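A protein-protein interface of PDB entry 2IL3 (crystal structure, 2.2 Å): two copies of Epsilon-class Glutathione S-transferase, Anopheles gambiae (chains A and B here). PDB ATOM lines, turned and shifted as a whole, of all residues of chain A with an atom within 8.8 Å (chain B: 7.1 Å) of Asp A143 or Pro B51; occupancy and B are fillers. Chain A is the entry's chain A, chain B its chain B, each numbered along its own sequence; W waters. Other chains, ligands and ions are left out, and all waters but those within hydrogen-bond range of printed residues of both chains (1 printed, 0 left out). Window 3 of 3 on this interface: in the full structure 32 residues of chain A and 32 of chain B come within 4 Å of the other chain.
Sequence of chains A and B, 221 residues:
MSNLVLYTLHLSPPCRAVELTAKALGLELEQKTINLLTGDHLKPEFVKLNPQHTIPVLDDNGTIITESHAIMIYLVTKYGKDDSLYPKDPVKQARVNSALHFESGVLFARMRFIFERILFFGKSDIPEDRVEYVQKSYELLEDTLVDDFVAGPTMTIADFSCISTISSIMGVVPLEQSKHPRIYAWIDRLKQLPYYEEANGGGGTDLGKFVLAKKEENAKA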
ATOM      1  N   ARG A  95      25.741 -15.585 -37.153  1.00  0.00           N
ATOM      2  CA  ARG A  95      25.434 -14.875 -35.926  1.00  0.00           C
ATOM      3  C   ARG A  95      25.257 -13.384 -36.146  1.00  0.00           C
ATOM      4  O   ARG A  95      24.362 -12.773 -35.632  1.00  0.00           O
ATOM      5  CB  ARG A  95      26.531 -15.090 -34.960  1.00  0.00           C
ATOM      6  CG  ARG A  95      26.203 -14.494 -33.602  1.00  0.00           C
ATOM      7  CD  ARG A  95      27.057 -15.223 -32.481  1.00  0.00           C
ATOM      8  NE  ARG A  95      26.713 -14.678 -31.156  1.00  0.00           N
ATOM      9  CZ  ARG A  95      27.542 -14.693 -30.099  1.00  0.00           C
ATOM     10  NH1 ARG A  95      27.164 -14.105 -28.963  1.00  0.00           N
ATOM     11  NH2 ARG A  95      28.775 -15.235 -30.172  1.00  0.00           N
ATOM     12  N   PHE A 102      17.032  -9.763 -36.276  1.00  0.00           N
ATOM     13  CA  PHE A 102      16.454  -9.497 -34.969  1.00  0.00           C
ATOM     14  C   PHE A 102      16.237  -7.970 -34.826  1.00  0.00           C
ATOM     15  O   PHE A 102      15.111  -7.475 -34.558  1.00  0.00           O
ATOM     16  CB  PHE A 102      17.384 -10.086 -33.861  1.00  0.00           C
ATOM     17  CG  PHE A 102      17.038  -9.547 -32.490  1.00  0.00           C
ATOM     18  CD1 PHE A 102      15.844  -9.948 -31.854  1.00  0.00           C
ATOM     19  CD2 PHE A 102      17.815  -8.524 -31.905  1.00  0.00           C
ATOM     20  CE1 PHE A 102      15.475  -9.347 -30.585  1.00  0.00           C
ATOM     21  CE2 PHE A 102      17.467  -7.957 -30.677  1.00  0.00           C
ATOM     22  CZ  PHE A 102      16.266  -8.395 -30.003  1.00  0.00           C
ATOM     23  N   LYS A 136       9.438  -5.829 -24.196  1.00  0.00           N
ATOM     24  CA  LYS A 136       9.840  -7.238 -24.515  1.00  0.00           C
ATOM     25  C   LYS A 136      11.051  -7.274 -25.454  1.00  0.00           C
ATOM     26  O   LYS A 136      11.953  -8.066 -25.278  1.00  0.00           O
ATOM     27  CB  LYS A 136       8.666  -8.101 -25.046  1.00  0.00           C
ATOM     28  CG  LYS A 136       8.113  -9.185 -23.989  1.00  0.00           C
ATOM     29  CD  LYS A 136       8.301 -10.802 -24.382  1.00  0.00           C
ATOM     30  CE  LYS A 136       9.700 -11.374 -25.004  1.00  0.00           C
ATOM     31  NZ  LYS A 136       9.550 -12.317 -26.266  1.00  0.00           N
ATOM     32  N   SER A 137      11.108  -6.328 -26.411  1.00  0.00           N
ATOM     33  CA  SER A 137      12.257  -6.190 -27.249  1.00  0.00           C
ATOM     34  C   SER A 137      13.555  -5.836 -26.492  1.00  0.00           C
ATOM     35  O   SER A 137      14.612  -6.416 -26.770  1.00  0.00           O
ATOM     36  CB  SER A 137      11.957  -5.311 -28.481  1.00  0.00           C
ATOM     37  OG  SER A 137      12.426  -4.004 -28.342  1.00  0.00           O
ATOM     38  N   TYR A 138      13.491  -4.930 -25.509  1.00  0.00           N
ATOM     39  CA  TYR A 138      14.625  -4.732 -24.609  1.00  0.00           C
ATOM     40  C   TYR A 138      15.135  -6.014 -23.928  1.00  0.00           C
ATOM     41  O   TYR A 138      16.324  -6.194 -23.806  1.00  0.00           O
ATOM     42  CB  TYR A 138      14.322  -3.710 -23.505  1.00  0.00           C
ATOM     43  CG  TYR A 138      13.915  -2.328 -23.950  1.00  0.00           C
ATOM     44  CD1 TYR A 138      14.347  -1.793 -25.207  1.00  0.00           C
ATOM     45  CD2 TYR A 138      13.225  -1.474 -23.068  1.00  0.00           C
ATOM     46  CE1 TYR A 138      14.100  -0.453 -25.564  1.00  0.00           C
ATOM     47  CE2 TYR A 138      12.940  -0.079 -23.445  1.00  0.00           C
ATOM     48  CZ  TYR A 138      13.435   0.404 -24.642  1.00  0.00           C
ATOM     49  OH  TYR A 138      13.133   1.644 -25.039  1.00  0.00           O
ATOM     50  N   GLU A 139      14.251  -6.857 -23.409  1.00  0.00           N
ATOM     51  CA  GLU A 139      14.646  -8.104 -22.682  1.00  0.00           C
ATOM     52  C   GLU A 139      15.236  -9.098 -23.655  1.00  0.00           C
ATOM     53  O   GLU A 139      16.103  -9.852 -23.304  1.00  0.00           O
ATOM     54  CB  GLU A 139      13.368  -8.744 -22.005  1.00  0.00           C
ATOM     55  CG  GLU A 139      13.543 -10.188 -21.409  1.00  0.00           C
ATOM     56  CD  GLU A 139      12.204 -10.956 -21.096  1.00  0.00           C
ATOM     57  OE1 GLU A 139      11.862 -12.037 -21.727  1.00  0.00           O
ATOM     58  OE2 GLU A 139      11.496 -10.466 -20.201  1.00  0.00           O
ATOM     59  N   LEU A 140      14.701  -9.154 -24.870  1.00  0.00           N
ATOM     60  CA  LEU A 140      15.218 -10.003 -25.879  1.00  0.00           C
ATOM     61  C   LEU A 140      16.646  -9.627 -26.257  1.00  0.00           C
ATOM     62  O   LEU A 140      17.382 -10.445 -26.777  1.00  0.00           O
ATOM     63  CB  LEU A 140      14.331  -9.864 -27.138  1.00  0.00           C
ATOM     64  CG  LEU A 140      13.016 -10.621 -27.188  1.00  0.00           C
ATOM     65  CD1 LEU A 140      12.168 -10.382 -28.480  1.00  0.00           C
ATOM     66  CD2 LEU A 140      13.368 -12.203 -26.977  1.00  0.00           C
ATOM     67  N   LEU A 141      16.987  -8.355 -26.108  1.00  0.00           N
ATOM     68  CA  LEU A 141      18.275  -7.853 -26.483  1.00  0.00           C
ATOM     69  C   LEU A 141      19.205  -8.114 -25.369  1.00  0.00           C
ATOM     70  O   LEU A 141      20.291  -8.550 -25.610  1.00  0.00           O
ATOM     71  CB  LEU A 141      18.241  -6.346 -26.802  1.00  0.00           C
ATOM     72  CG  LEU A 141      19.590  -5.578 -26.964  1.00  0.00           C
ATOM     73  CD1 LEU A 141      20.485  -6.234 -28.023  1.00  0.00           C
ATOM     74  CD2 LEU A 141      19.351  -4.102 -27.227  1.00  0.00           C
ATOM     75  N   GLU A 142      18.835  -7.775 -24.154  1.00  0.00           N
ATOM     76  CA  GLU A 142      19.627  -8.123 -22.946  1.00  0.00           C
ATOM     77  C   GLU A 142      20.009  -9.617 -22.873  1.00  0.00           C
ATOM     78  O   GLU A 142      21.142  -9.942 -22.587  1.00  0.00           O
ATOM     79  CB  GLU A 142      18.830  -7.648 -21.715  1.00  0.00           C
ATOM     80  CG  GLU A 142      19.349  -7.990 -20.351  1.00  0.00           C
ATOM     81  CD  GLU A 142      20.328  -7.079 -19.900  1.00  0.00           C
ATOM     82  OE1 GLU A 142      20.457  -5.965 -20.455  1.00  0.00           O
ATOM     83  OE2 GLU A 142      21.067  -7.502 -18.993  1.00  0.00           O
ATOM     84  N   ASP A 143      19.072 -10.528 -23.169  1.00  0.00           N
ATOM     85  CA  ASP A 143      19.395 -11.989 -23.383  1.00  0.00           C
ATOM     86  C   ASP A 143      20.253 -12.393 -24.585  1.00  0.00           C
ATOM     87  O   ASP A 143      20.768 -13.512 -24.627  1.00  0.00           O
ATOM     88  CB  ASP A 143      18.117 -12.833 -23.391  1.00  0.00           C
ATOM     89  CG  ASP A 143      17.329 -12.736 -22.061  1.00  0.00           C
ATOM     90  OD1 ASP A 143      16.174 -13.255 -22.023  1.00  0.00           O
ATOM     91  OD2 ASP A 143      17.843 -12.151 -21.063  1.00  0.00           O
ATOM     92  N   THR A 144      20.378 -11.514 -25.578  1.00  0.00           N
ATOM     93  CA  THR A 144      21.188 -11.789 -26.733  1.00  0.00           C
ATOM     94  C   THR A 144      22.635 -11.348 -26.445  1.00  0.00           C
ATOM     95  O   THR A 144      23.591 -11.862 -26.992  1.00  0.00           O
ATOM     96  CB  THR A 144      20.626 -11.047 -27.966  1.00  0.00           C
ATOM     97  OG1 THR A 144      19.277 -11.451 -28.163  1.00  0.00           O
ATOM     98  CG2 THR A 144      21.399 -11.416 -29.192  1.00  0.00           C
ATOM     99  N   LEU A 145      22.786 -10.446 -25.514  1.00  0.00           N
ATOM    100  CA  LEU A 145      24.114  -9.970 -25.104  1.00  0.00           C
ATOM    101  C   LEU A 145      24.840 -10.889 -24.063  1.00  0.00           C
ATOM    102  O   LEU A 145      25.211 -10.442 -22.978  1.00  0.00           O
ATOM    103  CB  LEU A 145      23.969  -8.516 -24.590  1.00  0.00           C
ATOM    104  CG  LEU A 145      23.897  -7.365 -25.617  1.00  0.00           C
ATOM    105  CD1 LEU A 145      23.319  -6.104 -24.929  1.00  0.00           C
ATOM    106  CD2 LEU A 145      25.258  -7.008 -26.199  1.00  0.00           C
ATOM    107  N   VAL A 146      25.035 -12.173 -24.390  1.00  0.00           N
ATOM    108  CA  VAL A 146      25.915 -13.078 -23.613  1.00  0.00           C
ATOM    109  C   VAL A 146      27.420 -12.753 -23.829  1.00  0.00           C
ATOM    110  O   VAL A 146      28.277 -12.942 -22.922  1.00  0.00           O
ATOM    111  CB  VAL A 146      25.630 -14.586 -23.904  1.00  0.00           C
ATOM    112  CG1 VAL A 146      24.182 -14.933 -23.559  1.00  0.00           C
ATOM    113  CG2 VAL A 146      25.909 -14.949 -25.348  1.00  0.00           C
ATOM    114  N   ASP A 147      27.719 -12.201 -25.008  1.00  0.00           N
ATOM    115  CA  ASP A 147      29.000 -11.582 -25.243  1.00  0.00           C
ATOM    116  C   ASP A 147      29.006 -10.068 -25.121  1.00  0.00           C
ATOM    117  O   ASP A 147      27.983  -9.439 -24.843  1.00  0.00           O
ATOM    118  CB  ASP A 147      29.526 -12.045 -26.598  1.00  0.00           C
ATOM    119  CG  ASP A 147      29.910 -13.551 -26.606  1.00  0.00           C
ATOM    120  OD1 ASP A 147      30.803 -13.951 -25.846  1.00  0.00           O
ATOM    121  OD2 ASP A 147      29.387 -14.344 -27.418  1.00  0.00           O
ATOM    122  N   VAL A 150      26.570  -7.573 -29.837  1.00  0.00           N
ATOM    123  CA  VAL A 150      25.345  -8.330 -30.052  1.00  0.00           C
ATOM    124  C   VAL A 150      25.536  -9.710 -30.741  1.00  0.00           C
ATOM    125  O   VAL A 150      24.756 -10.653 -30.439  1.00  0.00           O
ATOM    126  CB  VAL A 150      24.252  -7.566 -30.758  1.00  0.00           C
ATOM    127  CG1 VAL A 150      24.023  -6.331 -30.033  1.00  0.00           C
ATOM    128  CG2 VAL A 150      24.609  -7.291 -32.357  1.00  0.00           C
ATOM    129  N   LYS A 179      17.335  -3.494 -14.382  1.00  0.00           N
ATOM    130  CA  LYS A 179      16.843  -4.652 -15.125  1.00  0.00           C
ATOM    131  C   LYS A 179      17.602  -4.942 -16.434  1.00  0.00           C
ATOM    132  O   LYS A 179      17.504  -6.015 -16.990  1.00  0.00           O
ATOM    133  CB  LYS A 179      15.373  -4.423 -15.459  1.00  0.00           C
ATOM    134  CG  LYS A 179      14.437  -4.573 -14.281  1.00  0.00           C
ATOM    135  CD  LYS A 179      13.092  -5.114 -14.845  1.00  0.00           C
ATOM    136  CE  LYS A 179      11.894  -5.206 -13.861  1.00  0.00           C
ATOM    137  NZ  LYS A 179      11.225  -3.862 -13.712  1.00  0.00           N
ATOM    138  N   HIS A 180      18.313  -3.983 -16.972  1.00  0.00           N
ATOM    139  CA  HIS A 180      19.078  -4.259 -18.173  1.00  0.00           C
ATOM    140  C   HIS A 180      20.520  -3.865 -18.032  1.00  0.00           C
ATOM    141  O   HIS A 180      21.022  -3.062 -18.840  1.00  0.00           O
ATOM    142  CB  HIS A 180      18.422  -3.604 -19.437  1.00  0.00           C
ATOM    143  CG  HIS A 180      16.937  -3.856 -19.552  1.00  0.00           C
ATOM    144  ND1 HIS A 180      16.000  -3.101 -18.895  1.00  0.00           N
ATOM    145  CD2 HIS A 180      16.236  -4.756 -20.284  1.00  0.00           C
ATOM    146  CE1 HIS A 180      14.787  -3.560 -19.161  1.00  0.00           C
ATOM    147  NE2 HIS A 180      14.907  -4.565 -20.007  1.00  0.00           N
ATOM    148  N   ARG A 182      23.265  -5.448 -18.996  1.00  0.00           N
ATOM    149  CA  ARG A 182      24.016  -5.825 -20.169  1.00  0.00           C
ATOM    150  C   ARG A 182      23.887  -4.782 -21.323  1.00  0.00           C
ATOM    151  O   ARG A 182      24.900  -4.484 -22.018  1.00  0.00           O
ATOM    152  CB  ARG A 182      23.526  -7.147 -20.689  1.00  0.00           C
ATOM    153  CG  ARG A 182      24.128  -8.347 -19.978  1.00  0.00           C
ATOM    154  CD  ARG A 182      23.376  -9.544 -20.501  1.00  0.00           C
ATOM    155  NE  ARG A 182      23.987 -10.782 -20.060  1.00  0.00           N
ATOM    156  CZ  ARG A 182      23.486 -11.997 -20.276  1.00  0.00           C
ATOM    157  NH1 ARG A 182      22.339 -12.184 -20.993  1.00  0.00           N
ATOM    158  NH2 ARG A 182      24.130 -13.049 -19.752  1.00  0.00           N
ATOM    159  N   ILE A 183      22.658  -4.305 -21.569  1.00  0.00           N
ATOM    160  CA  ILE A 183      22.422  -3.275 -22.540  1.00  0.00           C
ATOM    161  C   ILE A 183      23.229  -2.046 -22.168  1.00  0.00           C
ATOM    162  O   ILE A 183      23.917  -1.469 -23.046  1.00  0.00           O
ATOM    163  CB  ILE A 183      20.855  -2.951 -22.698  1.00  0.00           C
ATOM    164  CG1 ILE A 183      20.080  -4.094 -23.393  1.00  0.00           C
ATOM    165  CG2 ILE A 183      20.603  -1.666 -23.441  1.00  0.00           C
ATOM    166  CD1 ILE A 183      18.555  -3.887 -23.203  1.00  0.00           C
ATOM    167  N   PHE B  46      15.392 -25.634 -24.254  1.00  0.00           N
ATOM    168  CA  PHE B  46      15.245 -24.809 -25.437  1.00  0.00           C
ATOM    169  C   PHE B  46      15.600 -23.349 -25.153  1.00  0.00           C
ATOM    170  O   PHE B  46      16.207 -22.661 -25.998  1.00  0.00           O
ATOM    171  CB  PHE B  46      13.823 -24.929 -25.993  1.00  0.00           C
ATOM    172  CG  PHE B  46      13.665 -24.338 -27.380  1.00  0.00           C
ATOM    173  CD1 PHE B  46      14.058 -25.071 -28.510  1.00  0.00           C
ATOM    174  CD2 PHE B  46      13.167 -23.035 -27.546  1.00  0.00           C
ATOM    175  CE1 PHE B  46      13.951 -24.518 -29.772  1.00  0.00           C
ATOM    176  CE2 PHE B  46      13.043 -22.469 -28.813  1.00  0.00           C
ATOM    177  CZ  PHE B  46      13.430 -23.197 -29.927  1.00  0.00           C
ATOM    178  N   VAL B  47      15.288 -22.882 -23.949  1.00  0.00           N
ATOM    179  CA  VAL B  47      15.588 -21.482 -23.564  1.00  0.00           C
ATOM    180  C   VAL B  47      17.065 -21.258 -23.420  1.00  0.00           C
ATOM    181  O   VAL B  47      17.537 -20.125 -23.516  1.00  0.00           O
ATOM    182  CB  VAL B  47      14.773 -20.990 -22.324  1.00  0.00           C
ATOM    183  CG1 VAL B  47      15.266 -19.629 -21.779  1.00  0.00           C
ATOM    184  CG2 VAL B  47      13.307 -20.903 -22.711  1.00  0.00           C
ATOM    185  N   LYS B  48      17.793 -22.357 -23.237  1.00  0.00           N
ATOM    186  CA  LYS B  48      19.213 -22.323 -23.108  1.00  0.00           C
ATOM    187  C   LYS B  48      19.798 -22.471 -24.521  1.00  0.00           C
ATOM    188  O   LYS B  48      20.867 -21.871 -24.891  1.00  0.00           O
ATOM    189  CB  LYS B  48      19.640 -23.438 -22.162  1.00  0.00           C
ATOM    190  CG  LYS B  48      21.164 -23.593 -21.918  1.00  0.00           C
ATOM    191  CD  LYS B  48      21.600 -25.079 -22.113  1.00  0.00           C
ATOM    192  CE  LYS B  48      21.148 -26.059 -20.976  1.00  0.00           C
ATOM    193  NZ  LYS B  48      20.753 -27.452 -21.488  1.00  0.00           N
ATOM    194  N   LEU B  49      19.077 -23.245 -25.326  1.00  0.00           N
ATOM    195  CA  LEU B  49      19.406 -23.334 -26.749  1.00  0.00           C
ATOM    196  C   LEU B  49      19.203 -21.998 -27.474  1.00  0.00           C
ATOM    197  O   LEU B  49      20.091 -21.504 -28.152  1.00  0.00           O
ATOM    198  CB  LEU B  49      18.579 -24.417 -27.456  1.00  0.00           C
ATOM    199  CG  LEU B  49      19.131 -24.944 -28.775  1.00  0.00           C
ATOM    200  CD1 LEU B  49      20.564 -25.486 -28.572  1.00  0.00           C
ATOM    201  CD2 LEU B  49      18.211 -26.023 -29.329  1.00  0.00           C
ATOM    202  N   ASN B  50      17.993 -21.458 -27.341  1.00  0.00           N
ATOM    203  CA  ASN B  50      17.643 -20.181 -27.977  1.00  0.00           C
ATOM    204  C   ASN B  50      17.210 -19.125 -26.970  1.00  0.00           C
ATOM    205  O   ASN B  50      16.052 -19.130 -26.577  1.00  0.00           O
ATOM    206  CB  ASN B  50      16.574 -20.399 -29.068  1.00  0.00           C
ATOM    207  CG  ASN B  50      16.197 -19.120 -29.802  1.00  0.00           C
ATOM    208  OD1 ASN B  50      15.296 -19.147 -30.639  1.00  0.00           O
ATOM    209  ND2 ASN B  50      16.847 -18.001 -29.483  1.00  0.00           N
ATOM    210  N   PRO B  51      18.147 -18.236 -26.545  1.00  0.00           N
ATOM    211  CA  PRO B  51      17.821 -17.130 -25.607  1.00  0.00           C
ATOM    212  C   PRO B  51      16.534 -16.308 -25.956  1.00  0.00           C
ATOM    213  O   PRO B  51      15.751 -15.950 -25.033  1.00  0.00           O
ATOM    214  CB  PRO B  51      19.110 -16.279 -25.562  1.00  0.00           C
ATOM    215  CG  PRO B  51      20.226 -17.337 -25.827  1.00  0.00           C
ATOM    216  CD  PRO B  51      19.584 -18.271 -26.881  1.00  0.00           C
ATOM    217  N   GLN B  52      16.306 -16.089 -27.263  1.00  0.00           N
ATOM    218  CA  GLN B  52      15.130 -15.340 -27.747  1.00  0.00           C
ATOM    219  C   GLN B  52      13.855 -16.150 -27.838  1.00  0.00           C
ATOM    220  O   GLN B  52      12.856 -15.604 -28.239  1.00  0.00           O
ATOM    221  CB  GLN B  52      15.430 -14.620 -29.058  1.00  0.00           C
ATOM    222  CG  GLN B  52      16.563 -13.580 -28.869  1.00  0.00           C
ATOM    223  CD  GLN B  52      17.132 -13.043 -30.147  1.00  0.00           C
ATOM    224  OE1 GLN B  52      18.244 -12.422 -30.178  1.00  0.00           O
ATOM    225  NE2 GLN B  52      16.417 -13.273 -31.226  1.00  0.00           N
ATOM    226  N   HIS B  53      13.904 -17.420 -27.387  1.00  0.00           N
ATOM    227  CA  HIS B  53      12.826 -18.415 -27.465  1.00  0.00           C
ATOM    228  C   HIS B  53      11.945 -18.461 -28.729  1.00  0.00           C
ATOM    229  O   HIS B  53      10.722 -18.581 -28.688  1.00  0.00           O
ATOM    230  CB  HIS B  53      12.003 -18.493 -26.176  1.00  0.00           C
ATOM    231  CG  HIS B  53      11.963 -17.227 -25.347  1.00  0.00           C
ATOM    232  ND1 HIS B  53      10.993 -16.251 -25.505  1.00  0.00           N
ATOM    233  CD2 HIS B  53      12.696 -16.848 -24.270  1.00  0.00           C
ATOM    234  CE1 HIS B  53      11.183 -15.293 -24.618  1.00  0.00           C
ATOM    235  NE2 HIS B  53      12.212 -15.629 -23.859  1.00  0.00           N
ATOM    236  N   THR B  54      12.574 -18.389 -29.883  1.00  0.00           N
ATOM    237  CA  THR B  54      11.827 -18.425 -31.139  1.00  0.00           C
ATOM    238  C   THR B  54      12.135 -19.719 -31.957  1.00  0.00           C
ATOM    239  O   THR B  54      13.015 -20.471 -31.594  1.00  0.00           O
ATOM    240  CB  THR B  54      12.147 -17.156 -31.988  1.00  0.00           C
ATOM    241  OG1 THR B  54      13.543 -17.132 -32.360  1.00  0.00           O
ATOM    242  CG2 THR B  54      11.815 -15.875 -31.211  1.00  0.00           C
ATOM    243  N   THR B  66      19.779 -19.476 -35.030  1.00  0.00           N
ATOM    244  CA  THR B  66      18.439 -19.182 -34.660  1.00  0.00           C
ATOM    245  C   THR B  66      18.053 -18.224 -35.829  1.00  0.00           C
ATOM    246  O   THR B  66      18.902 -17.957 -36.705  1.00  0.00           O
ATOM    247  CB  THR B  66      18.464 -18.648 -33.219  1.00  0.00           C
ATOM    248  OG1 THR B  66      19.257 -17.470 -33.146  1.00  0.00           O
ATOM    249  CG2 THR B  66      19.109 -19.733 -32.245  1.00  0.00           C
HETATM  250  O   HOH W   1      14.127 -12.984 -23.818  1.00  0.00           O
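OG1 of Thr A144 lies within hydrogen-bond range of OE1 of Gln B52.
O of Leu A140 lies within hydrogen-bond range of OG1 of Thr A144 (2.6 Å).
N of Gln B52 lies close to ND2 of Asn B50, at 3.0 Å.
Gln B52 touches Phe A102 (NE2 to CD1, 3.4 Å).
His B53 touches Lys A136.
CD2 of Leu A140 touches O of Gln B52, 3.7 Å away.
CB of Pro B51 touches O of Asp A143, at 3.4 Å.
Printed residues of chain B within 4 Å of Lys A136: His B53.
Glu A139 touches none of the printed residues of chain B.
Of chain B, only Pro B51 (3.4 Å) comes within 4 Å of Asp A143.
Val B47 touches none of the printed residues of chain A.
Pro B51 touches just one residue of chain A: Asp A143.
Printed residues of chain A within 4 Å of Gln B52: Phe A102, Leu A140 and Thr A144.
The nearest residue of chain B that does not touch Asp A143 is His B53 (5.0 Å).
The nearest printed residue of chain A that does not touch His B53 is Glu A139 (4.2 Å).
Hydrophobic or aromatic side chains of chain A within 4 Å of the printed part of chain B: Phe A102 and Leu A140.
Of the 10 printed residues of chain B, 3 touch a printed residue of chain A.
Hydrophobic or aromatic side chains of chain B that line the printed part of chain A: Pro B51 and His B53.
Among the printed residues, 5 pairs touch across the chains.
Among the printed residues, no Asp or Glu carboxylate lies within 4 Å of a Lys or Arg side-chain nitrogen of the other chain.
No position is printed for both chains.
Water W1 lies within hydrogen-bond range of OD1 of Asp A143, OE1 of Glu A139 and NE2 of His B53.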
